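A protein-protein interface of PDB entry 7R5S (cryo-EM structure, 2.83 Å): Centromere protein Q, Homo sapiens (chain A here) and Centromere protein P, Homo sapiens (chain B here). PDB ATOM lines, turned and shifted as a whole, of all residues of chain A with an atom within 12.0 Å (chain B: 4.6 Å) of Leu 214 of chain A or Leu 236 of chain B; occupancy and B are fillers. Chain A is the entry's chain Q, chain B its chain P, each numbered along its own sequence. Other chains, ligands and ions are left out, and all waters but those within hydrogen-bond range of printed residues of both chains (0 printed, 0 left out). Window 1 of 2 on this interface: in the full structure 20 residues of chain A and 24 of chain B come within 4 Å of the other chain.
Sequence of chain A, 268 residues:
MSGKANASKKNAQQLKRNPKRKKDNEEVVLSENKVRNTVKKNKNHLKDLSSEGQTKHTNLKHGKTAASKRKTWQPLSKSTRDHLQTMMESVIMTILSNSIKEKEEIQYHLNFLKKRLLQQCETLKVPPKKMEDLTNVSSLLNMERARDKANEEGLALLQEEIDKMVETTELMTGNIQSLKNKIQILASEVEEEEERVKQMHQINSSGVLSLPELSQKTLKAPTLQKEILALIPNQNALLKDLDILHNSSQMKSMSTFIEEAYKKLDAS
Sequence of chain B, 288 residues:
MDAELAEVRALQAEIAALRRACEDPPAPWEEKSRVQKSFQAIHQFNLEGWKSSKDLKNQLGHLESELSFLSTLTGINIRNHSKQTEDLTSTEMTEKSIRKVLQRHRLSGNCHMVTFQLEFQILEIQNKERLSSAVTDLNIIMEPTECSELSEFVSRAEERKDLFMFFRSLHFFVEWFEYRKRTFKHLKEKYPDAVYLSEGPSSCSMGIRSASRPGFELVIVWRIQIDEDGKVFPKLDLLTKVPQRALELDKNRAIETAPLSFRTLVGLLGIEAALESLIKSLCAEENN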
ATOM      1  N   LEU A 209      11.387  13.846  40.491  1.00  0.00           N
ATOM      2  CA  LEU A 209      10.396  12.970  39.879  1.00  0.00           C
ATOM      3  C   LEU A 209      11.064  11.955  38.957  1.00  0.00           C
ATOM      4  O   LEU A 209      11.265  12.216  37.772  1.00  0.00           O
ATOM      5  CB  LEU A 209       9.359  13.784  39.102  1.00  0.00           C
ATOM      6  CG  LEU A 209       8.387  14.651  39.908  1.00  0.00           C
ATOM      7  CD1 LEU A 209       8.983  16.020  40.209  1.00  0.00           C
ATOM      8  CD2 LEU A 209       7.059  14.788  39.178  1.00  0.00           C
ATOM      9  N   SER A 210      11.407  10.792  39.512  1.00  0.00           N
ATOM     10  CA  SER A 210      12.054   9.728  38.745  1.00  0.00           C
ATOM     11  C   SER A 210      10.993   8.764  38.212  1.00  0.00           C
ATOM     12  O   SER A 210      10.830   7.633  38.672  1.00  0.00           O
ATOM     13  CB  SER A 210      13.089   9.010  39.602  1.00  0.00           C
ATOM     14  OG  SER A 210      12.578   8.732  40.893  1.00  0.00           O
ATOM     15  N   LEU A 211      10.261   9.244  37.213  1.00  0.00           N
ATOM     16  CA  LEU A 211       9.213   8.444  36.594  1.00  0.00           C
ATOM     17  C   LEU A 211       9.812   7.552  35.513  1.00  0.00           C
ATOM     18  O   LEU A 211      10.486   8.062  34.611  1.00  0.00           O
ATOM     19  CB  LEU A 211       8.137   9.340  35.998  1.00  0.00           C
ATOM     20  CG  LEU A 211       7.385  10.245  36.975  1.00  0.00           C
ATOM     21  CD1 LEU A 211       6.361  11.095  36.239  1.00  0.00           C
ATOM     22  CD2 LEU A 211       6.718   9.422  38.066  1.00  0.00           C
ATOM     23  N   PRO A 212       9.606   6.237  35.569  1.00  0.00           N
ATOM     24  CA  PRO A 212      10.136   5.365  34.515  1.00  0.00           C
ATOM     25  C   PRO A 212       9.495   5.673  33.170  1.00  0.00           C
ATOM     26  O   PRO A 212       8.308   5.996  33.084  1.00  0.00           O
ATOM     27  CB  PRO A 212       9.775   3.956  35.002  1.00  0.00           C
ATOM     28  CG  PRO A 212       9.535   4.103  36.472  1.00  0.00           C
ATOM     29  CD  PRO A 212       8.960   5.474  36.648  1.00  0.00           C
ATOM     30  N   GLU A 213      10.297   5.572  32.114  1.00  0.00           N
ATOM     31  CA  GLU A 213       9.808   5.862  30.775  1.00  0.00           C
ATOM     32  C   GLU A 213       8.893   4.746  30.284  1.00  0.00           C
ATOM     33  O   GLU A 213       9.147   3.562  30.521  1.00  0.00           O
ATOM     34  CB  GLU A 213      10.979   6.043  29.810  1.00  0.00           C
ATOM     35  CG  GLU A 213      10.588   6.619  28.459  1.00  0.00           C
ATOM     36  CD  GLU A 213       9.853   7.939  28.580  1.00  0.00           C
ATOM     37  OE1 GLU A 213      10.348   8.832  29.298  1.00  0.00           O
ATOM     38  OE2 GLU A 213       8.780   8.085  27.958  1.00  0.00           O
ATOM     39  N   LEU A 214       7.821   5.134  29.600  1.00  0.00           N
ATOM     40  CA  LEU A 214       6.887   4.161  29.052  1.00  0.00           C
ATOM     41  C   LEU A 214       7.517   3.416  27.881  1.00  0.00           C
ATOM     42  O   LEU A 214       8.308   3.971  27.113  1.00  0.00           O
ATOM     43  CB  LEU A 214       5.592   4.845  28.602  1.00  0.00           C
ATOM     44  CG  LEU A 214       4.576   5.323  29.647  1.00  0.00           C
ATOM     45  CD1 LEU A 214       5.128   6.418  30.547  1.00  0.00           C
ATOM     46  CD2 LEU A 214       3.300   5.795  28.964  1.00  0.00           C
ATOM     47  N   SER A 215       7.159   2.142  27.754  1.00  0.00           N
ATOM     48  CA  SER A 215       7.698   1.316  26.687  1.00  0.00           C
ATOM     49  C   SER A 215       7.096   1.713  25.341  1.00  0.00           C
ATOM     50  O   SER A 215       6.094   2.429  25.262  1.00  0.00           O
ATOM     51  CB  SER A 215       7.429  -0.163  26.964  1.00  0.00           C
ATOM     52  OG  SER A 215       6.166  -0.554  26.453  1.00  0.00           O
ATOM     53  N   GLN A 216       7.729   1.233  24.269  1.00  0.00           N
ATOM     54  CA  GLN A 216       7.248   1.516  22.923  1.00  0.00           C
ATOM     55  C   GLN A 216       5.910   0.857  22.622  1.00  0.00           C
ATOM     56  O   GLN A 216       5.233   1.279  21.678  1.00  0.00           O
ATOM     57  CB  GLN A 216       8.288   1.074  21.890  1.00  0.00           C
ATOM     58  CG  GLN A 216       8.341   1.951  20.647  1.00  0.00           C
ATOM     59  CD  GLN A 216       9.061   3.267  20.882  1.00  0.00           C
ATOM     60  OE1 GLN A 216       9.555   3.532  21.978  1.00  0.00           O
ATOM     61  NE2 GLN A 216       9.121   4.099  19.849  1.00  0.00           N
ATOM     62  N   LYS A 217       5.518  -0.164  23.389  1.00  0.00           N
ATOM     63  CA  LYS A 217       4.197  -0.758  23.209  1.00  0.00           C
ATOM     64  C   LYS A 217       3.099   0.256  23.501  1.00  0.00           C
ATOM     65  O   LYS A 217       2.059   0.270  22.831  1.00  0.00           O
ATOM     66  CB  LYS A 217       4.051  -1.987  24.105  1.00  0.00           C
ATOM     67  CG  LYS A 217       2.677  -2.638  24.060  1.00  0.00           C
ATOM     68  CD  LYS A 217       2.559  -3.747  25.094  1.00  0.00           C
ATOM     69  CE  LYS A 217       2.773  -3.214  26.501  1.00  0.00           C
ATOM     70  NZ  LYS A 217       2.649  -4.285  27.527  1.00  0.00           N
ATOM     71  N   THR A 218       3.317   1.117  24.497  1.00  0.00           N
ATOM     72  CA  THR A 218       2.356   2.176  24.787  1.00  0.00           C
ATOM     73  C   THR A 218       2.360   3.240  23.697  1.00  0.00           C
ATOM     74  O   THR A 218       1.301   3.755  23.321  1.00  0.00           O
ATOM     75  CB  THR A 218       2.665   2.807  26.145  1.00  0.00           C
ATOM     76  OG1 THR A 218       2.918   1.776  27.107  1.00  0.00           O
ATOM     77  CG2 THR A 218       1.504   3.662  26.607  1.00  0.00           C
ATOM     78  N   LEU A 219       3.541   3.581  23.178  1.00  0.00           N
ATOM     79  CA  LEU A 219       3.632   4.630  22.169  1.00  0.00           C
ATOM     80  C   LEU A 219       3.085   4.169  20.825  1.00  0.00           C
ATOM     81  O   LEU A 219       2.653   4.999  20.016  1.00  0.00           O
ATOM     82  CB  LEU A 219       5.082   5.089  22.024  1.00  0.00           C
ATOM     83  CG  LEU A 219       5.801   5.452  23.325  1.00  0.00           C
ATOM     84  CD1 LEU A 219       7.216   5.925  23.040  1.00  0.00           C
ATOM     85  CD2 LEU A 219       5.024   6.511  24.091  1.00  0.00           C
ATOM     86  N   LYS A 220       3.093   2.863  20.567  1.00  0.00           N
ATOM     87  CA  LYS A 220       2.582   2.308  19.322  1.00  0.00           C
ATOM     88  C   LYS A 220       1.190   1.710  19.480  1.00  0.00           C
ATOM     89  O   LYS A 220       0.679   1.096  18.537  1.00  0.00           O
ATOM     90  CB  LYS A 220       3.548   1.253  18.780  1.00  0.00           C
ATOM     91  CG  LYS A 220       4.936   1.791  18.472  1.00  0.00           C
ATOM     92  CD  LYS A 220       4.875   2.981  17.526  1.00  0.00           C
ATOM     93  CE  LYS A 220       6.264   3.516  17.222  1.00  0.00           C
ATOM     94  NZ  LYS A 220       6.218   4.700  16.321  1.00  0.00           N
ATOM     95  N   ALA A 221       0.569   1.873  20.645  1.00  0.00           N
ATOM     96  CA  ALA A 221      -0.774   1.371  20.859  1.00  0.00           C
ATOM     97  C   ALA A 221      -1.781   2.200  20.066  1.00  0.00           C
ATOM     98  O   ALA A 221      -1.529   3.365  19.750  1.00  0.00           O
ATOM     99  CB  ALA A 221      -1.118   1.401  22.346  1.00  0.00           C
ATOM    100  N   PRO A 222      -2.929   1.616  19.722  1.00  0.00           N
ATOM    101  CA  PRO A 222      -3.960   2.388  19.016  1.00  0.00           C
ATOM    102  C   PRO A 222      -4.478   3.535  19.873  1.00  0.00           C
ATOM    103  O   PRO A 222      -4.927   3.337  21.005  1.00  0.00           O
ATOM    104  CB  PRO A 222      -5.050   1.347  18.733  1.00  0.00           C
ATOM    105  CG  PRO A 222      -4.794   0.241  19.703  1.00  0.00           C
ATOM    106  CD  PRO A 222      -3.311   0.202  19.879  1.00  0.00           C
ATOM    107  N   THR A 223      -4.412   4.745  19.322  1.00  0.00           N
ATOM    108  CA  THR A 223      -4.781   5.936  20.072  1.00  0.00           C
ATOM    109  C   THR A 223      -6.294   6.011  20.275  1.00  0.00           C
ATOM    110  O   THR A 223      -7.073   5.264  19.679  1.00  0.00           O
ATOM    111  CB  THR A 223      -4.277   7.198  19.368  1.00  0.00           C
ATOM    112  OG1 THR A 223      -4.760   8.357  20.058  1.00  0.00           O
ATOM    113  CG2 THR A 223      -4.752   7.237  17.929  1.00  0.00           C
ATOM    114  N   LEU A 224      -6.701   6.941  21.141  1.00  0.00           N
ATOM    115  CA  LEU A 224      -8.085   7.009  21.598  1.00  0.00           C
ATOM    116  C   LEU A 224      -8.989   7.741  20.611  1.00  0.00           C
ATOM    117  O   LEU A 224     -10.142   7.337  20.407  1.00  0.00           O
ATOM    118  CB  LEU A 224      -8.137   7.688  22.968  1.00  0.00           C
ATOM    119  CG  LEU A 224      -9.511   7.955  23.582  1.00  0.00           C
ATOM    120  CD1 LEU A 224     -10.256   6.649  23.785  1.00  0.00           C
ATOM    121  CD2 LEU A 224      -9.385   8.720  24.894  1.00  0.00           C
ATOM    122  N   GLN A 225      -8.490   8.814  19.990  1.00  0.00           N
ATOM    123  CA  GLN A 225      -9.364   9.687  19.211  1.00  0.00           C
ATOM    124  C   GLN A 225      -9.919   8.979  17.981  1.00  0.00           C
ATOM    125  O   GLN A 225     -11.115   9.086  17.683  1.00  0.00           O
ATOM    126  CB  GLN A 225      -8.618  10.956  18.800  1.00  0.00           C
ATOM    127  CG  GLN A 225      -9.508  11.993  18.135  1.00  0.00           C
ATOM    128  CD  GLN A 225      -8.739  13.204  17.653  1.00  0.00           C
ATOM    129  OE1 GLN A 225      -7.516  13.168  17.529  1.00  0.00           O
ATOM    130  NE2 GLN A 225      -9.455  14.288  17.379  1.00  0.00           N
ATOM    131  N   LYS A 226      -9.069   8.259  17.246  1.00  0.00           N
ATOM    132  CA  LYS A 226      -9.539   7.590  16.036  1.00  0.00           C
ATOM    133  C   LYS A 226     -10.499   6.458  16.379  1.00  0.00           C
ATOM    134  O   LYS A 226     -11.471   6.213  15.658  1.00  0.00           O
ATOM    135  CB  LYS A 226      -8.358   7.067  15.220  1.00  0.00           C
ATOM    136  CG  LYS A 226      -7.469   6.101  15.971  1.00  0.00           C
ATOM    137  CD  LYS A 226      -6.806   5.121  15.020  1.00  0.00           C
ATOM    138  CE  LYS A 226      -5.774   4.270  15.737  1.00  0.00           C
ATOM    139  NZ  LYS A 226      -6.267   3.824  17.065  1.00  0.00           N
ATOM    140  N   GLU A 227     -10.236   5.751  17.482  1.00  0.00           N
ATOM    141  CA  GLU A 227     -11.159   4.711  17.924  1.00  0.00           C
ATOM    142  C   GLU A 227     -12.518   5.301  18.268  1.00  0.00           C
ATOM    143  O   GLU A 227     -13.556   4.754  17.881  1.00  0.00           O
ATOM    144  CB  GLU A 227     -10.581   3.960  19.124  1.00  0.00           C
ATOM    145  CG  GLU A 227      -9.348   3.128  18.816  1.00  0.00           C
ATOM    146  CD  GLU A 227      -8.741   2.509  20.061  1.00  0.00           C
ATOM    147  OE1 GLU A 227      -8.986   3.031  21.168  1.00  0.00           O
ATOM    148  OE2 GLU A 227      -8.021   1.496  19.933  1.00  0.00           O
ATOM    149  N   ILE A 228     -12.530   6.430  18.980  1.00  0.00           N
ATOM    150  CA  ILE A 228     -13.793   7.083  19.311  1.00  0.00           C
ATOM    151  C   ILE A 228     -14.516   7.520  18.043  1.00  0.00           C
ATOM    152  O   ILE A 228     -15.725   7.311  17.896  1.00  0.00           O
ATOM    153  CB  ILE A 228     -13.553   8.272  20.260  1.00  0.00           C
ATOM    154  CG1 ILE A 228     -13.179   7.775  21.657  1.00  0.00           C
ATOM    155  CG2 ILE A 228     -14.787   9.161  20.326  1.00  0.00           C
ATOM    156  CD1 ILE A 228     -13.013   8.887  22.673  1.00  0.00           C
ATOM    157  N   TRP B 176       1.424   2.300  39.869  1.00  0.00           N
ATOM    158  CA  TRP B 176       1.110   3.220  38.779  1.00  0.00           C
ATOM    159  C   TRP B 176       0.062   4.247  39.195  1.00  0.00           C
ATOM    160  O   TRP B 176       0.115   5.402  38.751  1.00  0.00           O
ATOM    161  CB  TRP B 176       0.643   2.444  37.548  1.00  0.00           C
ATOM    162  CG  TRP B 176       1.763   2.077  36.625  1.00  0.00           C
ATOM    163  CD1 TRP B 176       2.302   0.838  36.443  1.00  0.00           C
ATOM    164  CD2 TRP B 176       2.492   2.962  35.767  1.00  0.00           C
ATOM    165  NE1 TRP B 176       3.318   0.895  35.518  1.00  0.00           N
ATOM    166  CE2 TRP B 176       3.454   2.188  35.089  1.00  0.00           C
ATOM    167  CE3 TRP B 176       2.422   4.334  35.504  1.00  0.00           C
ATOM    168  CZ2 TRP B 176       4.339   2.740  34.165  1.00  0.00           C
ATOM    169  CZ3 TRP B 176       3.301   4.879  34.586  1.00  0.00           C
ATOM    170  CH2 TRP B 176       4.247   4.083  33.929  1.00  0.00           C
ATOM    171  N   VAL B 221      -5.499  12.447  28.628  1.00  0.00           N
ATOM    172  CA  VAL B 221      -6.095  11.246  29.201  1.00  0.00           C
ATOM    173  C   VAL B 221      -4.978  10.323  29.665  1.00  0.00           C
ATOM    174  O   VAL B 221      -4.040  10.047  28.910  1.00  0.00           O
ATOM    175  CB  VAL B 221      -7.007  10.533  28.187  1.00  0.00           C
ATOM    176  CG1 VAL B 221      -7.574   9.258  28.786  1.00  0.00           C
ATOM    177  CG2 VAL B 221      -8.118  11.462  27.724  1.00  0.00           C
ATOM    178  N   TRP B 222      -5.083   9.848  30.906  1.00  0.00           N
ATOM    179  CA  TRP B 222      -4.132   8.900  31.476  1.00  0.00           C
ATOM    180  C   TRP B 222      -4.924   7.750  32.083  1.00  0.00           C
ATOM    181  O   TRP B 222      -5.623   7.936  33.085  1.00  0.00           O
ATOM    182  CB  TRP B 222      -3.241   9.569  32.524  1.00  0.00           C
ATOM    183  CG  TRP B 222      -2.022   8.774  32.893  1.00  0.00           C
ATOM    184  CD1 TRP B 222      -1.817   7.440  32.686  1.00  0.00           C
ATOM    185  CD2 TRP B 222      -0.837   9.266  33.529  1.00  0.00           C
ATOM    186  NE1 TRP B 222      -0.581   7.072  33.157  1.00  0.00           N
ATOM    187  CE2 TRP B 222       0.041   8.175  33.679  1.00  0.00           C
ATOM    188  CE3 TRP B 222      -0.435  10.524  33.988  1.00  0.00           C
ATOM    189  CZ2 TRP B 222       1.296   8.304  34.268  1.00  0.00           C
ATOM    190  CZ3 TRP B 222       0.812  10.649  34.572  1.00  0.00           C
ATOM    191  CH2 TRP B 222       1.663   9.546  34.707  1.00  0.00           C
ATOM    192  N   PRO B 234       0.248   1.419  31.226  1.00  0.00           N
ATOM    193  CA  PRO B 234      -0.594   2.613  31.082  1.00  0.00           C
ATOM    194  C   PRO B 234      -0.822   2.995  29.628  1.00  0.00           C
ATOM    195  O   PRO B 234      -0.425   2.263  28.717  1.00  0.00           O
ATOM    196  CB  PRO B 234       0.205   3.688  31.824  1.00  0.00           C
ATOM    197  CG  PRO B 234       1.626   3.274  31.626  1.00  0.00           C
ATOM    198  CD  PRO B 234       1.638   1.762  31.576  1.00  0.00           C
ATOM    199  N   LYS B 235      -1.473   4.135  29.404  1.00  0.00           N
ATOM    200  CA  LYS B 235      -1.686   4.654  28.060  1.00  0.00           C
ATOM    201  C   LYS B 235      -1.938   6.152  28.150  1.00  0.00           C
ATOM    202  O   LYS B 235      -2.652   6.613  29.043  1.00  0.00           O
ATOM    203  CB  LYS B 235      -2.857   3.951  27.364  1.00  0.00           C
ATOM    204  CG  LYS B 235      -4.111   3.830  28.211  1.00  0.00           C
ATOM    205  CD  LYS B 235      -5.300   3.391  27.373  1.00  0.00           C
ATOM    206  CE  LYS B 235      -4.980   2.145  26.561  1.00  0.00           C
ATOM    207  NZ  LYS B 235      -4.553   1.012  27.426  1.00  0.00           N
ATOM    208  N   LEU B 236      -1.347   6.902  27.221  1.00  0.00           N
ATOM    209  CA  LEU B 236      -1.418   8.360  27.221  1.00  0.00           C
ATOM    210  C   LEU B 236      -1.947   8.838  25.879  1.00  0.00           C
ATOM    211  O   LEU B 236      -1.339   8.569  24.838  1.00  0.00           O
ATOM    212  CB  LEU B 236      -0.046   8.977  27.506  1.00  0.00           C
ATOM    213  CG  LEU B 236       0.457   8.888  28.947  1.00  0.00           C
ATOM    214  CD1 LEU B 236       1.878   9.412  29.051  1.00  0.00           C
ATOM    215  CD2 LEU B 236      -0.468   9.657  29.876  1.00  0.00           C
ATOM    216  N   ASP B 237      -3.076   9.543  25.905  1.00  0.00           N
ATOM    217  CA  ASP B 237      -3.676  10.138  24.719  1.00  0.00           C
ATOM    218  C   ASP B 237      -4.147  11.547  25.059  1.00  0.00           C
ATOM    219  O   ASP B 237      -4.085  11.986  26.213  1.00  0.00           O
ATOM    220  CB  ASP B 237      -4.841   9.287  24.198  1.00  0.00           C
ATOM    221  CG  ASP B 237      -4.524   7.806  24.184  1.00  0.00           C
ATOM    222  OD1 ASP B 237      -4.547   7.184  25.267  1.00  0.00           O
ATOM    223  OD2 ASP B 237      -4.253   7.263  23.093  1.00  0.00           O
ATOM    224  N   PHE B 262       2.109  14.139  19.384  1.00  0.00           N
ATOM    225  CA  PHE B 262       2.247  14.283  20.831  1.00  0.00           C
ATOM    226  C   PHE B 262       2.877  13.043  21.447  1.00  0.00           C
ATOM    227  O   PHE B 262       3.736  13.148  22.330  1.00  0.00           O
ATOM    228  CB  PHE B 262       0.888  14.560  21.471  1.00  0.00           C
ATOM    229  CG  PHE B 262       0.816  14.191  22.926  1.00  0.00           C
ATOM    230  CD1 PHE B 262       1.423  14.983  23.886  1.00  0.00           C
ATOM    231  CD2 PHE B 262       0.137  13.054  23.333  1.00  0.00           C
ATOM    232  CE1 PHE B 262       1.358  14.647  25.225  1.00  0.00           C
ATOM    233  CE2 PHE B 262       0.068  12.713  24.672  1.00  0.00           C
ATOM    234  CZ  PHE B 262       0.679  13.511  25.619  1.00  0.00           C
ATOM    235  N   ARG B 263       2.465  11.858  20.991  1.00  0.00           N
ATOM    236  CA  ARG B 263       3.077  10.632  21.485  1.00  0.00           C
ATOM    237  C   ARG B 263       4.569  10.616  21.177  1.00  0.00           C
ATOM    238  O   ARG B 263       5.391  10.300  22.045  1.00  0.00           O
ATOM    239  CB  ARG B 263       2.371   9.416  20.885  1.00  0.00           C
ATOM    240  CG  ARG B 263       0.865   9.439  21.097  1.00  0.00           C
ATOM    241  CD  ARG B 263       0.291   8.043  21.252  1.00  0.00           C
ATOM    242  NE  ARG B 263       0.324   7.297  19.998  1.00  0.00           N
ATOM    243  CZ  ARG B 263      -0.244   6.109  19.824  1.00  0.00           C
ATOM    244  NH1 ARG B 263      -0.895   5.531  20.824  1.00  0.00           N
ATOM    245  NH2 ARG B 263      -0.164   5.500  18.649  1.00  0.00           N
ATOM    246  N   VAL B 266       6.128  12.561  23.828  1.00  0.00           N
ATOM    247  CA  VAL B 266       6.336  11.857  25.088  1.00  0.00           C
ATOM    248  C   VAL B 266       7.292  10.690  24.882  1.00  0.00           C
ATOM    249  O   VAL B 266       7.856  10.168  25.851  1.00  0.00           O
ATOM    250  CB  VAL B 266       4.994  11.408  25.711  1.00  0.00           C
ATOM    251  CG1 VAL B 266       4.278  10.402  24.837  1.00  0.00           C
ATOM    252  CG2 VAL B 266       5.188  10.867  27.122  1.00  0.00           C
ATOM    253  N   ILE B 271       7.712  12.203  30.118  1.00  0.00           N
ATOM    254  CA  ILE B 271       6.278  12.427  30.264  1.00  0.00           C
ATOM    255  C   ILE B 271       6.036  13.820  30.828  1.00  0.00           C
ATOM    256  O   ILE B 271       5.396  14.661  30.186  1.00  0.00           O
ATOM    257  CB  ILE B 271       5.633  11.358  31.166  1.00  0.00           C
ATOM    258  CG1 ILE B 271       5.987   9.952  30.678  1.00  0.00           C
ATOM    259  CG2 ILE B 271       4.125  11.548  31.223  1.00  0.00           C
ATOM    260  CD1 ILE B 271       7.144   9.315  31.425  1.00  0.00           C
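Ser 210 of chain A touches none of the printed residues of chain B.
Of the printed residues of chain B, Pro 212 of chain A touches Ile 271.
Of the printed residues of chain B, Thr 218 of chain A touches Pro 234, Lys 235 and Arg 263.
Of the printed residues of chain B, Leu 219 of chain A touches Arg 263.
Of the printed residues of chain B, Thr 223 of chain A touches Asp 237 (3.3 Å) and Arg 263 (3.9 Å).
Trp 176 of chain B touches none of the printed residues of chain A.
No residue of chain A comes within 4 Å of Trp 222 of chain B.
Pro 234 of chain B touches just one residue of chain A: Thr 218 (3.2 Å).
Leu 236 of chain B touches one residue of chain A.
Of chain A, only Thr 223 (3.3 Å) and Leu 224 (3.1 Å) come within 4 Å of Asp 237 of chain B.
Val 266 of chain B touches just one residue of chain A: Glu 213 (3.1 Å).
Printed residues of chain A within 4 Å of Ile 271 of chain B: Pro 212, Glu 213 and Leu 214.
The nearest residue of chain A that does not touch Leu 236 of chain B is Thr 218 of chain A (4.4 Å).
O of Pro 212 of chain A touches CD1 of Ile 271 of chain B (3.9 Å).
Ile 271 of chain B touches Glu 213 of chain A.
Leu 214 of chain A touches Leu 236 of chain B (CD2 to CD1, 3.9 Å).
Leu 214 of chain A touches Ile 271 of chain B (CD1 to CD1, 3.6 Å).
O of Pro 234 of chain B touches CG2 of Thr 218 of chain A, at 3.2 Å.
CA of Lys 235 of chain B touches CG2 of Thr 218 of chain A (3.6 Å).
NH1 of Arg 263 of chain B touches O of Thr 218 of chain A, 3.8 Å away.
NH1 of Arg 263 of chain B touches N of Thr 223 of chain A, 3.9 Å away.
Of the 20 printed residues of chain A, 8 touch a printed residue of chain B.
Along chain A the printed residues that touch a printed residue of chain B span positions 212 to 224.
Of the 11 printed residues of chain B, 7 touch a printed residue of chain A.
Among the printed residues, no Asp or Glu carboxylate lies within 4 Å of a Lys or Arg side-chain nitrogen of the other chain.
The guanidinium group (NH1) of Arg 263 of chain B is in hydrogen-bond range of the backbone carbonyl oxygen (O) of Ala 221 of chain A, at 2.5 Å.
OG1 of Thr 223 of chain A lies within hydrogen-bond range of OD2 of Asp 237 of chain B, at 3.3 Å.
The backbone carbonyl oxygen (O) of Leu 219 of chain A sits close to the guanidinium group (NH2) of Arg 263 of chain B (3.2 Å).
N of Leu 224 of chain A is in hydrogen-bond range of OD2 of Asp 237 of chain B, at 3.1 Å.
OE2 of Glu 213 of chain A sits close to O of Val 266 of chain B.
The backbone NH (N) of Val 221 of chain B lies within hydrogen-bond range of the backbone carbonyl oxygen (O) of Asp 237 of chain B, at 2.8 Å.
The backbone carbonyl oxygen of Thr 223 of chain A is in hydrogen-bond range of the side-chain amino group of Lys 226 of chain A, at 3.1 Å.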
